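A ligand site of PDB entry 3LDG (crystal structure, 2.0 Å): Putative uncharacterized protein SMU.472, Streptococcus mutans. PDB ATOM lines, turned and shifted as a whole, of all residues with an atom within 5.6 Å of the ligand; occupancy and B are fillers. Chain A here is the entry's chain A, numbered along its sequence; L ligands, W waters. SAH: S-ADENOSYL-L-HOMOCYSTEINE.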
ATOM      1  N   ARG A 170      -4.364   7.340 -19.582  1.00  0.00           N
ATOM      2  CA  ARG A 170      -3.714   8.592 -19.176  1.00  0.00           C
ATOM      3  C   ARG A 170      -3.801   8.784 -17.664  1.00  0.00           C
ATOM      4  O   ARG A 170      -4.891   8.885 -17.114  1.00  0.00           O
ATOM      5  CB  ARG A 170      -4.342   9.784 -19.902  1.00  0.00           C
ATOM      6  CG  ARG A 170      -3.519  11.052 -19.805  1.00  0.00           C
ATOM      7  CD  ARG A 170      -3.929  12.070 -20.854  1.00  0.00           C
ATOM      8  NE  ARG A 170      -3.551  11.675 -22.214  1.00  0.00           N
ATOM      9  CZ  ARG A 170      -2.313  11.731 -22.685  1.00  0.00           C
ATOM     10  NH1 ARG A 170      -1.320  12.148 -21.914  1.00  0.00           N
ATOM     11  NH2 ARG A 170      -2.048  11.367 -23.933  1.00  0.00           N
ATOM     12  N   ALA A 176      -0.518  19.697 -20.978  1.00  0.00           N
ATOM     13  CA  ALA A 176      -0.985  19.942 -22.344  1.00  0.00           C
ATOM     14  C   ALA A 176      -0.578  18.834 -23.315  1.00  0.00           C
ATOM     15  O   ALA A 176       0.060  19.097 -24.331  1.00  0.00           O
ATOM     16  CB  ALA A 176      -0.491  21.298 -22.844  1.00  0.00           C
ATOM     17  N   PRO A 177      -0.961  17.592 -22.996  1.00  0.00           N
ATOM     18  CA  PRO A 177      -0.707  16.491 -23.927  1.00  0.00           C
ATOM     19  C   PRO A 177      -1.505  16.736 -25.198  1.00  0.00           C
ATOM     20  O   PRO A 177      -2.624  17.237 -25.122  1.00  0.00           O
ATOM     21  CB  PRO A 177      -1.277  15.272 -23.199  1.00  0.00           C
ATOM     22  CG  PRO A 177      -1.689  15.752 -21.823  1.00  0.00           C
ATOM     23  CD  PRO A 177      -1.878  17.216 -21.915  1.00  0.00           C
ATOM     24  N   ILE A 178      -0.939  16.417 -26.344  1.00  0.00           N
ATOM     25  CA  ILE A 178      -1.759  16.333 -27.527  1.00  0.00           C
ATOM     26  C   ILE A 178      -2.822  15.268 -27.235  1.00  0.00           C
ATOM     27  O   ILE A 178      -2.549  14.302 -26.527  1.00  0.00           O
ATOM     28  CB  ILE A 178      -0.911  15.944 -28.738  1.00  0.00           C
ATOM     29  CG1 ILE A 178      -1.637  16.268 -30.038  1.00  0.00           C
ATOM     30  CG2 ILE A 178      -0.509  14.486 -28.666  1.00  0.00           C
ATOM     31  CD1 ILE A 178      -0.744  16.055 -31.258  1.00  0.00           C
ATOM     32  N   ASP A 200       9.668   8.882 -31.381  1.00  0.00           N
ATOM     33  CA  ASP A 200       9.201  10.198 -30.970  1.00  0.00           C
ATOM     34  C   ASP A 200      10.256  10.832 -30.097  1.00  0.00           C
ATOM     35  O   ASP A 200      10.440  10.420 -28.948  1.00  0.00           O
ATOM     36  CB  ASP A 200       7.873  10.107 -30.191  1.00  0.00           C
ATOM     37  CG  ASP A 200       7.318  11.486 -29.803  1.00  0.00           C
ATOM     38  OD1 ASP A 200       8.060  12.492 -29.819  1.00  0.00           O
ATOM     39  OD2 ASP A 200       6.125  11.571 -29.458  1.00  0.00           O
ATOM     40  N   PRO A 201      10.976  11.835 -30.626  1.00  0.00           N
ATOM     41  CA  PRO A 201      12.138  12.412 -29.931  1.00  0.00           C
ATOM     42  C   PRO A 201      11.789  13.542 -28.973  1.00  0.00           C
ATOM     43  O   PRO A 201      12.698  14.107 -28.366  1.00  0.00           O
ATOM     44  CB  PRO A 201      12.951  12.983 -31.085  1.00  0.00           C
ATOM     45  CG  PRO A 201      11.827  13.618 -31.947  1.00  0.00           C
ATOM     46  CD  PRO A 201      10.823  12.434 -31.978  1.00  0.00           C
ATOM     47  N   THR A 202      10.504  13.869 -28.856  1.00  0.00           N
ATOM     48  CA  THR A 202      10.017  14.831 -27.891  1.00  0.00           C
ATOM     49  C   THR A 202       8.772  14.266 -27.205  1.00  0.00           C
ATOM     50  O   THR A 202       7.705  14.851 -27.264  1.00  0.00           O
ATOM     51  CB  THR A 202       9.653  16.152 -28.589  1.00  0.00           C
ATOM     52  OG1 THR A 202       8.753  15.876 -29.671  1.00  0.00           O
ATOM     53  CG2 THR A 202      10.893  16.832 -29.145  1.00  0.00           C
ATOM     54  N   CYS A 203       8.918  13.111 -26.545  1.00  0.00           N
ATOM     55  CA  CYS A 203       7.767  12.222 -26.373  1.00  0.00           C
ATOM     56  C   CYS A 203       6.753  12.663 -25.342  1.00  0.00           C
ATOM     57  O   CYS A 203       5.642  12.148 -25.307  1.00  0.00           O
ATOM     58  CB  CYS A 203       8.206  10.765 -26.122  1.00  0.00           C
ATOM     59  SG  CYS A 203       8.983  10.456 -24.491  1.00  0.00           S
ATOM     60  N   GLY A 204       7.129  13.624 -24.493  1.00  0.00           N
ATOM     61  CA  GLY A 204       6.222  14.062 -23.448  1.00  0.00           C
ATOM     62  C   GLY A 204       5.679  12.877 -22.682  1.00  0.00           C
ATOM     63  O   GLY A 204       6.450  12.015 -22.237  1.00  0.00           O
ATOM     64  N   SER A 205       4.355  12.815 -22.551  1.00  0.00           N
ATOM     65  CA  SER A 205       3.674  11.754 -21.799  1.00  0.00           C
ATOM     66  C   SER A 205       3.506  10.406 -22.518  1.00  0.00           C
ATOM     67  O   SER A 205       2.804   9.521 -22.013  1.00  0.00           O
ATOM     68  CB  SER A 205       2.299  12.253 -21.368  1.00  0.00           C
ATOM     69  OG  SER A 205       1.513  12.488 -22.523  1.00  0.00           O
ATOM     70  N   GLY A 206       4.110  10.265 -23.697  1.00  0.00           N
ATOM     71  CA  GLY A 206       4.185   8.980 -24.392  1.00  0.00           C
ATOM     72  C   GLY A 206       3.065   8.670 -25.389  1.00  0.00           C
ATOM     73  O   GLY A 206       2.951   7.543 -25.856  1.00  0.00           O
ATOM     74  N   THR A 207       2.250   9.666 -25.693  1.00  0.00           N
ATOM     75  CA  THR A 207       1.025   9.504 -26.495  1.00  0.00           C
ATOM     76  C   THR A 207       1.293   8.941 -27.896  1.00  0.00           C
ATOM     77  O   THR A 207       0.638   8.009 -28.339  1.00  0.00           O
ATOM     78  CB  THR A 207       0.333  10.868 -26.652  1.00  0.00           C
ATOM     79  OG1 THR A 207       0.355  11.536 -25.390  1.00  0.00           O
ATOM     80  CG2 THR A 207      -1.094  10.683 -27.141  1.00  0.00           C
ATOM     81  N   PHE A 208       2.260   9.512 -28.600  1.00  0.00           N
ATOM     82  CA  PHE A 208       2.600   9.003 -29.929  1.00  0.00           C
ATOM     83  C   PHE A 208       3.043   7.536 -29.872  1.00  0.00           C
ATOM     84  O   PHE A 208       2.570   6.709 -30.643  1.00  0.00           O
ATOM     85  CB  PHE A 208       3.623   9.907 -30.619  1.00  0.00           C
ATOM     86  CG  PHE A 208       3.008  11.122 -31.257  1.00  0.00           C
ATOM     87  CD1 PHE A 208       2.208  11.001 -32.390  1.00  0.00           C
ATOM     88  CD2 PHE A 208       3.202  12.388 -30.720  1.00  0.00           C
ATOM     89  CE1 PHE A 208       1.621  12.132 -32.990  1.00  0.00           C
ATOM     90  CE2 PHE A 208       2.616  13.514 -31.304  1.00  0.00           C
ATOM     91  CZ  PHE A 208       1.836  13.379 -32.441  1.00  0.00           C
ATOM     92  N   PHE A 262      11.659   9.521 -26.409  1.00  0.00           N
ATOM     93  CA  PHE A 262      12.461  10.113 -25.364  1.00  0.00           C
ATOM     94  C   PHE A 262      12.119  11.587 -25.242  1.00  0.00           C
ATOM     95  O   PHE A 262      11.427  12.140 -26.108  1.00  0.00           O
ATOM     96  CB  PHE A 262      13.949   9.885 -25.626  1.00  0.00           C
ATOM     97  CG  PHE A 262      14.373  10.104 -27.055  1.00  0.00           C
ATOM     98  CD1 PHE A 262      14.711  11.375 -27.503  1.00  0.00           C
ATOM     99  CD2 PHE A 262      14.454   9.034 -27.945  1.00  0.00           C
ATOM    100  CE1 PHE A 262      15.115  11.568 -28.837  1.00  0.00           C
ATOM    101  CE2 PHE A 262      14.852   9.235 -29.259  1.00  0.00           C
ATOM    102  CZ  PHE A 262      15.183  10.500 -29.697  1.00  0.00           C
ATOM    103  N   ASP A 263      12.583  12.200 -24.162  1.00  0.00           N
ATOM    104  CA  ASP A 263      12.269  13.574 -23.792  1.00  0.00           C
ATOM    105  C   ASP A 263      13.367  14.039 -22.844  1.00  0.00           C
ATOM    106  O   ASP A 263      13.841  13.253 -22.016  1.00  0.00           O
ATOM    107  CB  ASP A 263      10.924  13.615 -23.062  1.00  0.00           C
ATOM    108  CG  ASP A 263      10.368  15.014 -22.932  1.00  0.00           C
ATOM    109  OD1 ASP A 263      11.009  15.859 -22.272  1.00  0.00           O
ATOM    110  OD2 ASP A 263       9.295  15.270 -23.510  1.00  0.00           O
ATOM    111  N   PHE A 264      13.803  15.290 -22.959  1.00  0.00           N
ATOM    112  CA  PHE A 264      14.860  15.741 -22.085  1.00  0.00           C
ATOM    113  C   PHE A 264      14.358  16.095 -20.692  1.00  0.00           C
ATOM    114  O   PHE A 264      15.143  16.534 -19.853  1.00  0.00           O
ATOM    115  CB  PHE A 264      15.636  16.916 -22.714  1.00  0.00           C
ATOM    116  CG  PHE A 264      14.977  18.260 -22.525  1.00  0.00           C
ATOM    117  CD1 PHE A 264      15.752  19.416 -22.480  1.00  0.00           C
ATOM    118  CD2 PHE A 264      13.599  18.373 -22.426  1.00  0.00           C
ATOM    119  CE1 PHE A 264      15.154  20.677 -22.325  1.00  0.00           C
ATOM    120  CE2 PHE A 264      12.980  19.630 -22.260  1.00  0.00           C
ATOM    121  CZ  PHE A 264      13.767  20.775 -22.211  1.00  0.00           C
ATOM    122  N   ASP A 265      13.057  15.925 -20.447  1.00  0.00           N
ATOM    123  CA  ASP A 265      12.471  16.186 -19.118  1.00  0.00           C
ATOM    124  C   ASP A 265      12.126  14.871 -18.395  1.00  0.00           C
ATOM    125  O   ASP A 265      11.202  14.140 -18.794  1.00  0.00           O
ATOM    126  CB  ASP A 265      11.233  17.080 -19.250  1.00  0.00           C
ATOM    127  CG  ASP A 265      10.620  17.472 -17.893  1.00  0.00           C
ATOM    128  OD1 ASP A 265      11.049  16.991 -16.843  1.00  0.00           O
ATOM    129  OD2 ASP A 265       9.668  18.267 -17.911  1.00  0.00           O
ATOM    130  N   MET A 268       8.517  14.048 -17.480  1.00  0.00           N
ATOM    131  CA  MET A 268       7.668  13.560 -18.545  1.00  0.00           C
ATOM    132  C   MET A 268       7.896  12.068 -18.795  1.00  0.00           C
ATOM    133  O   MET A 268       6.949  11.307 -18.999  1.00  0.00           O
ATOM    134  CB  MET A 268       7.871  14.355 -19.841  1.00  0.00           C
ATOM    135  CG  MET A 268       7.604  15.855 -19.689  1.00  0.00           C
ATOM    136  SD  MET A 268       5.731  16.165 -19.132  1.00  0.00           S
ATOM    137  CE  MET A 268       4.907  15.051 -20.448  1.00  0.00           C
ATOM    138  N   MET A 290      16.341  11.621 -22.572  1.00  0.00           N
ATOM    139  CA  MET A 290      17.491  12.011 -23.397  1.00  0.00           C
ATOM    140  C   MET A 290      17.175  13.287 -24.173  1.00  0.00           C
ATOM    141  O   MET A 290      16.026  13.496 -24.583  1.00  0.00           O
ATOM    142  CB  MET A 290      17.847  10.905 -24.402  1.00  0.00           C
ATOM    143  CG  MET A 290      19.165  11.173 -25.172  1.00  0.00           C
ATOM    144  SD  MET A 290      19.613   9.771 -26.505  1.00  0.00           S
ATOM    145  CE  MET A 290      18.100   9.939 -27.689  1.00  0.00           C
ATOM    146  N   ARG A 291      18.197  14.124 -24.398  1.00  0.00           N
ATOM    147  CA  ARG A 291      18.074  15.263 -25.319  1.00  0.00           C
ATOM    148  C   ARG A 291      18.009  14.730 -26.743  1.00  0.00           C
ATOM    149  O   ARG A 291      18.769  13.819 -27.097  1.00  0.00           O
ATOM    150  CB  ARG A 291      19.278  16.204 -25.205  1.00  0.00           C
ATOM    151  CG  ARG A 291      19.442  16.827 -23.831  1.00  0.00           C
ATOM    152  CD  ARG A 291      20.770  17.585 -23.718  1.00  0.00           C
ATOM    153  NE  ARG A 291      20.910  18.621 -24.736  1.00  0.00           N
ATOM    154  CZ  ARG A 291      21.799  18.616 -25.723  1.00  0.00           C
ATOM    155  NH1 ARG A 291      22.681  17.621 -25.850  1.00  0.00           N
ATOM    156  NH2 ARG A 291      21.830  19.625 -26.585  1.00  0.00           N
ATOM    157  N   LEU A 292      17.127  15.282 -27.570  1.00  0.00           N
ATOM    158  CA  LEU A 292      17.031  14.776 -28.933  1.00  0.00           C
ATOM    159  C   LEU A 292      18.304  15.033 -29.740  1.00  0.00           C
ATOM    160  O   LEU A 292      18.577  14.358 -30.735  1.00  0.00           O
ATOM    161  CB  LEU A 292      15.800  15.352 -29.665  1.00  0.00           C
ATOM    162  CG  LEU A 292      15.774  16.865 -29.872  1.00  0.00           C
ATOM    163  CD1 LEU A 292      16.557  17.241 -31.094  1.00  0.00           C
ATOM    164  CD2 LEU A 292      14.352  17.350 -30.016  1.00  0.00           C
ATOM    165  N   GLN A 293      19.071  16.027 -29.307  1.00  0.00           N
ATOM    166  CA  GLN A 293      20.316  16.385 -29.998  1.00  0.00           C
ATOM    167  C   GLN A 293      21.356  15.267 -29.963  1.00  0.00           C
ATOM    168  O   GLN A 293      22.294  15.243 -30.765  1.00  0.00           O
ATOM    169  CB  GLN A 293      20.905  17.671 -29.433  1.00  0.00           C
ATOM    170  CG  GLN A 293      20.012  18.916 -29.665  1.00  0.00           C
ATOM    171  CD  GLN A 293      19.024  19.144 -28.511  1.00  0.00           C
ATOM    172  OE1 GLN A 293      18.647  18.216 -27.795  1.00  0.00           O
ATOM    173  NE2 GLN A 293      18.612  20.406 -28.341  1.00  0.00           N
ATOM    174  N   ASN A 307       6.117  16.338 -31.876  1.00  0.00           N
ATOM    175  CA  ASN A 307       5.312  17.522 -31.546  1.00  0.00           C
ATOM    176  C   ASN A 307       6.188  18.414 -30.658  1.00  0.00           C
ATOM    177  O   ASN A 307       6.032  18.398 -29.449  1.00  0.00           O
ATOM    178  CB  ASN A 307       4.058  17.100 -30.746  1.00  0.00           C
ATOM    179  CG  ASN A 307       3.118  18.281 -30.427  1.00  0.00           C
ATOM    180  OD1 ASN A 307       3.003  19.226 -31.208  1.00  0.00           O
ATOM    181  ND2 ASN A 307       2.448  18.209 -29.284  1.00  0.00           N
ATOM    182  N   PRO A 308       7.148  19.154 -31.259  1.00  0.00           N
ATOM    183  CA  PRO A 308       8.138  19.868 -30.442  1.00  0.00           C
ATOM    184  C   PRO A 308       7.576  21.125 -29.788  1.00  0.00           C
ATOM    185  O   PRO A 308       6.442  21.503 -30.089  1.00  0.00           O
ATOM    186  CB  PRO A 308       9.228  20.242 -31.461  1.00  0.00           C
ATOM    187  CG  PRO A 308       8.508  20.343 -32.752  1.00  0.00           C
ATOM    188  CD  PRO A 308       7.503  19.183 -32.694  1.00  0.00           C
ATOM    189  N   PRO A 309       8.339  21.743 -28.878  1.00  0.00           N
ATOM    190  CA  PRO A 309       7.919  23.041 -28.312  1.00  0.00           C
ATOM    191  C   PRO A 309       7.493  24.003 -29.422  1.00  0.00           C
ATOM    192  O   PRO A 309       8.171  24.166 -30.441  1.00  0.00           O
ATOM    193  CB  PRO A 309       9.188  23.550 -27.629  1.00  0.00           C
ATOM    194  CG  PRO A 309       9.924  22.290 -27.220  1.00  0.00           C
ATOM    195  CD  PRO A 309       9.573  21.236 -28.248  1.00  0.00           C
ATOM    196  N   LEU A 323      16.511  25.390 -31.134  1.00  0.00           N
ATOM    197  CA  LEU A 323      15.973  24.042 -31.012  1.00  0.00           C
ATOM    198  C   LEU A 323      15.657  23.463 -32.390  1.00  0.00           C
ATOM    199  O   LEU A 323      16.107  22.368 -32.732  1.00  0.00           O
ATOM    200  CB  LEU A 323      14.708  24.048 -30.161  1.00  0.00           C
ATOM    201  CG  LEU A 323      14.048  22.668 -30.010  1.00  0.00           C
ATOM    202  CD1 LEU A 323      15.034  21.683 -29.391  1.00  0.00           C
ATOM    203  CD2 LEU A 323      12.772  22.773 -29.158  1.00  0.00           C
HETATM  204  N   SAH L   1       3.201  15.218 -27.674  1.00  0.00           N
HETATM  205  CA  SAH L   1       3.479  15.179 -26.234  1.00  0.00           C
HETATM  206  CB  SAH L   1       3.912  16.549 -25.681  1.00  0.00           C
HETATM  207  CG  SAH L   1       4.947  17.288 -26.545  1.00  0.00           C
HETATM  208  SD  SAH L   1       5.356  18.916 -25.830  1.00  0.00           S
HETATM  209  C   SAH L   1       2.348  14.555 -25.398  1.00  0.00           C
HETATM  210  O   SAH L   1       2.524  14.321 -24.209  1.00  0.00           O
HETATM  211  OXT SAH L   1       1.245  14.260 -25.879  1.00  0.00           O
HETATM  212  C5' SAH L   1       7.065  18.936 -26.347  1.00  0.00           C
HETATM  213  C4' SAH L   1       7.985  18.044 -25.500  1.00  0.00           C
HETATM  214  O4' SAH L   1       9.303  18.197 -25.984  1.00  0.00           O
HETATM  215  C3' SAH L   1       8.017  18.359 -24.007  1.00  0.00           C
HETATM  216  O3' SAH L   1       7.605  17.208 -23.235  1.00  0.00           O
HETATM  217  C2' SAH L   1       9.470  18.762 -23.755  1.00  0.00           C
HETATM  218  O2' SAH L   1      10.005  18.339 -22.531  1.00  0.00           O
HETATM  219  C1' SAH L   1      10.188  18.052 -24.909  1.00  0.00           C
HETATM  220  N9  SAH L   1      11.496  18.612 -25.257  1.00  0.00           N
HETATM  221  C8  SAH L   1      11.852  19.947 -25.284  1.00  0.00           C
HETATM  222  N7  SAH L   1      13.139  20.035 -25.664  1.00  0.00           N
HETATM  223  C5  SAH L   1      13.636  18.782 -25.875  1.00  0.00           C
HETATM  224  C6  SAH L   1      14.901  18.301 -26.257  1.00  0.00           C
HETATM  225  N6  SAH L   1      15.933  19.121 -26.523  1.00  0.00           N
HETATM  226  N1  SAH L   1      15.076  16.927 -26.381  1.00  0.00           N
HETATM  227  C2  SAH L   1      14.043  16.047 -26.131  1.00  0.00           C
HETATM  228  N3  SAH L   1      12.801  16.538 -25.746  1.00  0.00           N
HETATM  229  C4  SAH L   1      12.602  17.884 -25.617  1.00  0.00           C
HETATM  230  O   HOH W   1      17.074  21.735 -26.043  1.00  0.00           O
HETATM  231  O   HOH W   2       9.092  19.555 -20.331  1.00  0.00           O
HETATM  232  O   HOH W   3      11.445  23.204 -24.095  1.00  0.00           O
HETATM  233  O   HOH W   4      13.495  22.742 -25.618  1.00  0.00           O
HETATM  234  O   HOH W   5       4.214  20.976 -28.185  1.00  0.00           O
HETATM  235  O   HOH W   6       2.494  16.347 -22.251  1.00  0.00           O
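An oxygen (O3') of the ligand sits at hydrogen-bond distance from the side-chain carboxylate (OD2) of Asp 263, 2.6 Å away.
The backbone NH (N) of Ser 205 is in hydrogen-bond range of an oxygen (O) of the ligand (2.9 Å).
An oxygen (O) of the ligand sits at hydrogen-bond distance from the side-chain hydroxyl (OG) of Ser 205, 2.7 Å away.
A nitrogen (N1) of the ligand sits at hydrogen-bond distance from the backbone NH of Leu 292, at 2.9 Å.
An oxygen (OXT) of the ligand lies within hydrogen-bond range of the side-chain hydroxyl (OG1) of Thr 207 (2.9 Å).
The backbone NH (N) of Ile 178 lies within hydrogen-bond range of an oxygen (OXT) of the ligand, 3.1 Å away.
A nitrogen (N6) of the ligand is in hydrogen-bond range of the side-chain amide oxygen (OE1) of Gln 293, at 3.1 Å.
N of Phe 264 sits at hydrogen-bond distance from N3 of the ligand (3.2 Å).
A nitrogen (N) of the ligand lies close to the side-chain amide nitrogen (ND2) of Asn 307 (3.5 Å).
The side-chain carboxylate of Asp 263 is in hydrogen-bond range of the backbone NH of Gly 204.
The side-chain carboxylate (OD1) of Asp 263 is in hydrogen-bond range of the backbone NH (N) of Asp 265, 2.7 Å away.
OG of Ser 205 is in hydrogen-bond range of NH1 of Arg 170.
The backbone carbonyl oxygen of Met 290 is in hydrogen-bond range of the backbone NH of Phe 264 (3.3 Å).
N of Asn 307 lies within hydrogen-bond range of OG1 of Thr 202.
N of Thr 202 lies within hydrogen-bond range of O of Phe 262 (3.4 Å).
The backbone NH of Thr 202 is in hydrogen-bond range of the side-chain carboxylate of Asp 200 (3.0 Å).
N of Cys 203 sits at hydrogen-bond distance from O of Phe 262 (2.7 Å).
CA of Pro 177 touches OXT of the ligand, at 3.5 Å.
Pro 201 touches the ligand (O to C2, 3.3 Å).
CB of Thr 202 touches O4' of the ligand, at 3.3 Å.
Cys 203 touches the ligand.
CA of Gly 204 touches O3' of the ligand (3.4 Å).
Asp 265 touches the ligand (CB to O2', 3.7 Å).
Met 268 touches the ligand (CG to O3', 3.8 Å).
Met 290 touches the ligand.
CA of Arg 291 touches N1 of the ligand, at 3.6 Å.
CG of Pro 309 touches C8 of the ligand, 3.6 Å away.
CD1 of Leu 323 touches N6 of the ligand, at 3.9 Å.
The nearest printed residue that does not touch the ligand is Phe 208 (4.1 Å).
Water W2 lies within hydrogen-bond range of O2' of the ligand (2.7 Å) and OD2 of Asp 265 (2.8 Å).
Water W1 bridges a nitrogen (N6) of the ligand (2.9 Å) and the side-chain amide nitrogen of Gln 293 (3.1 Å).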
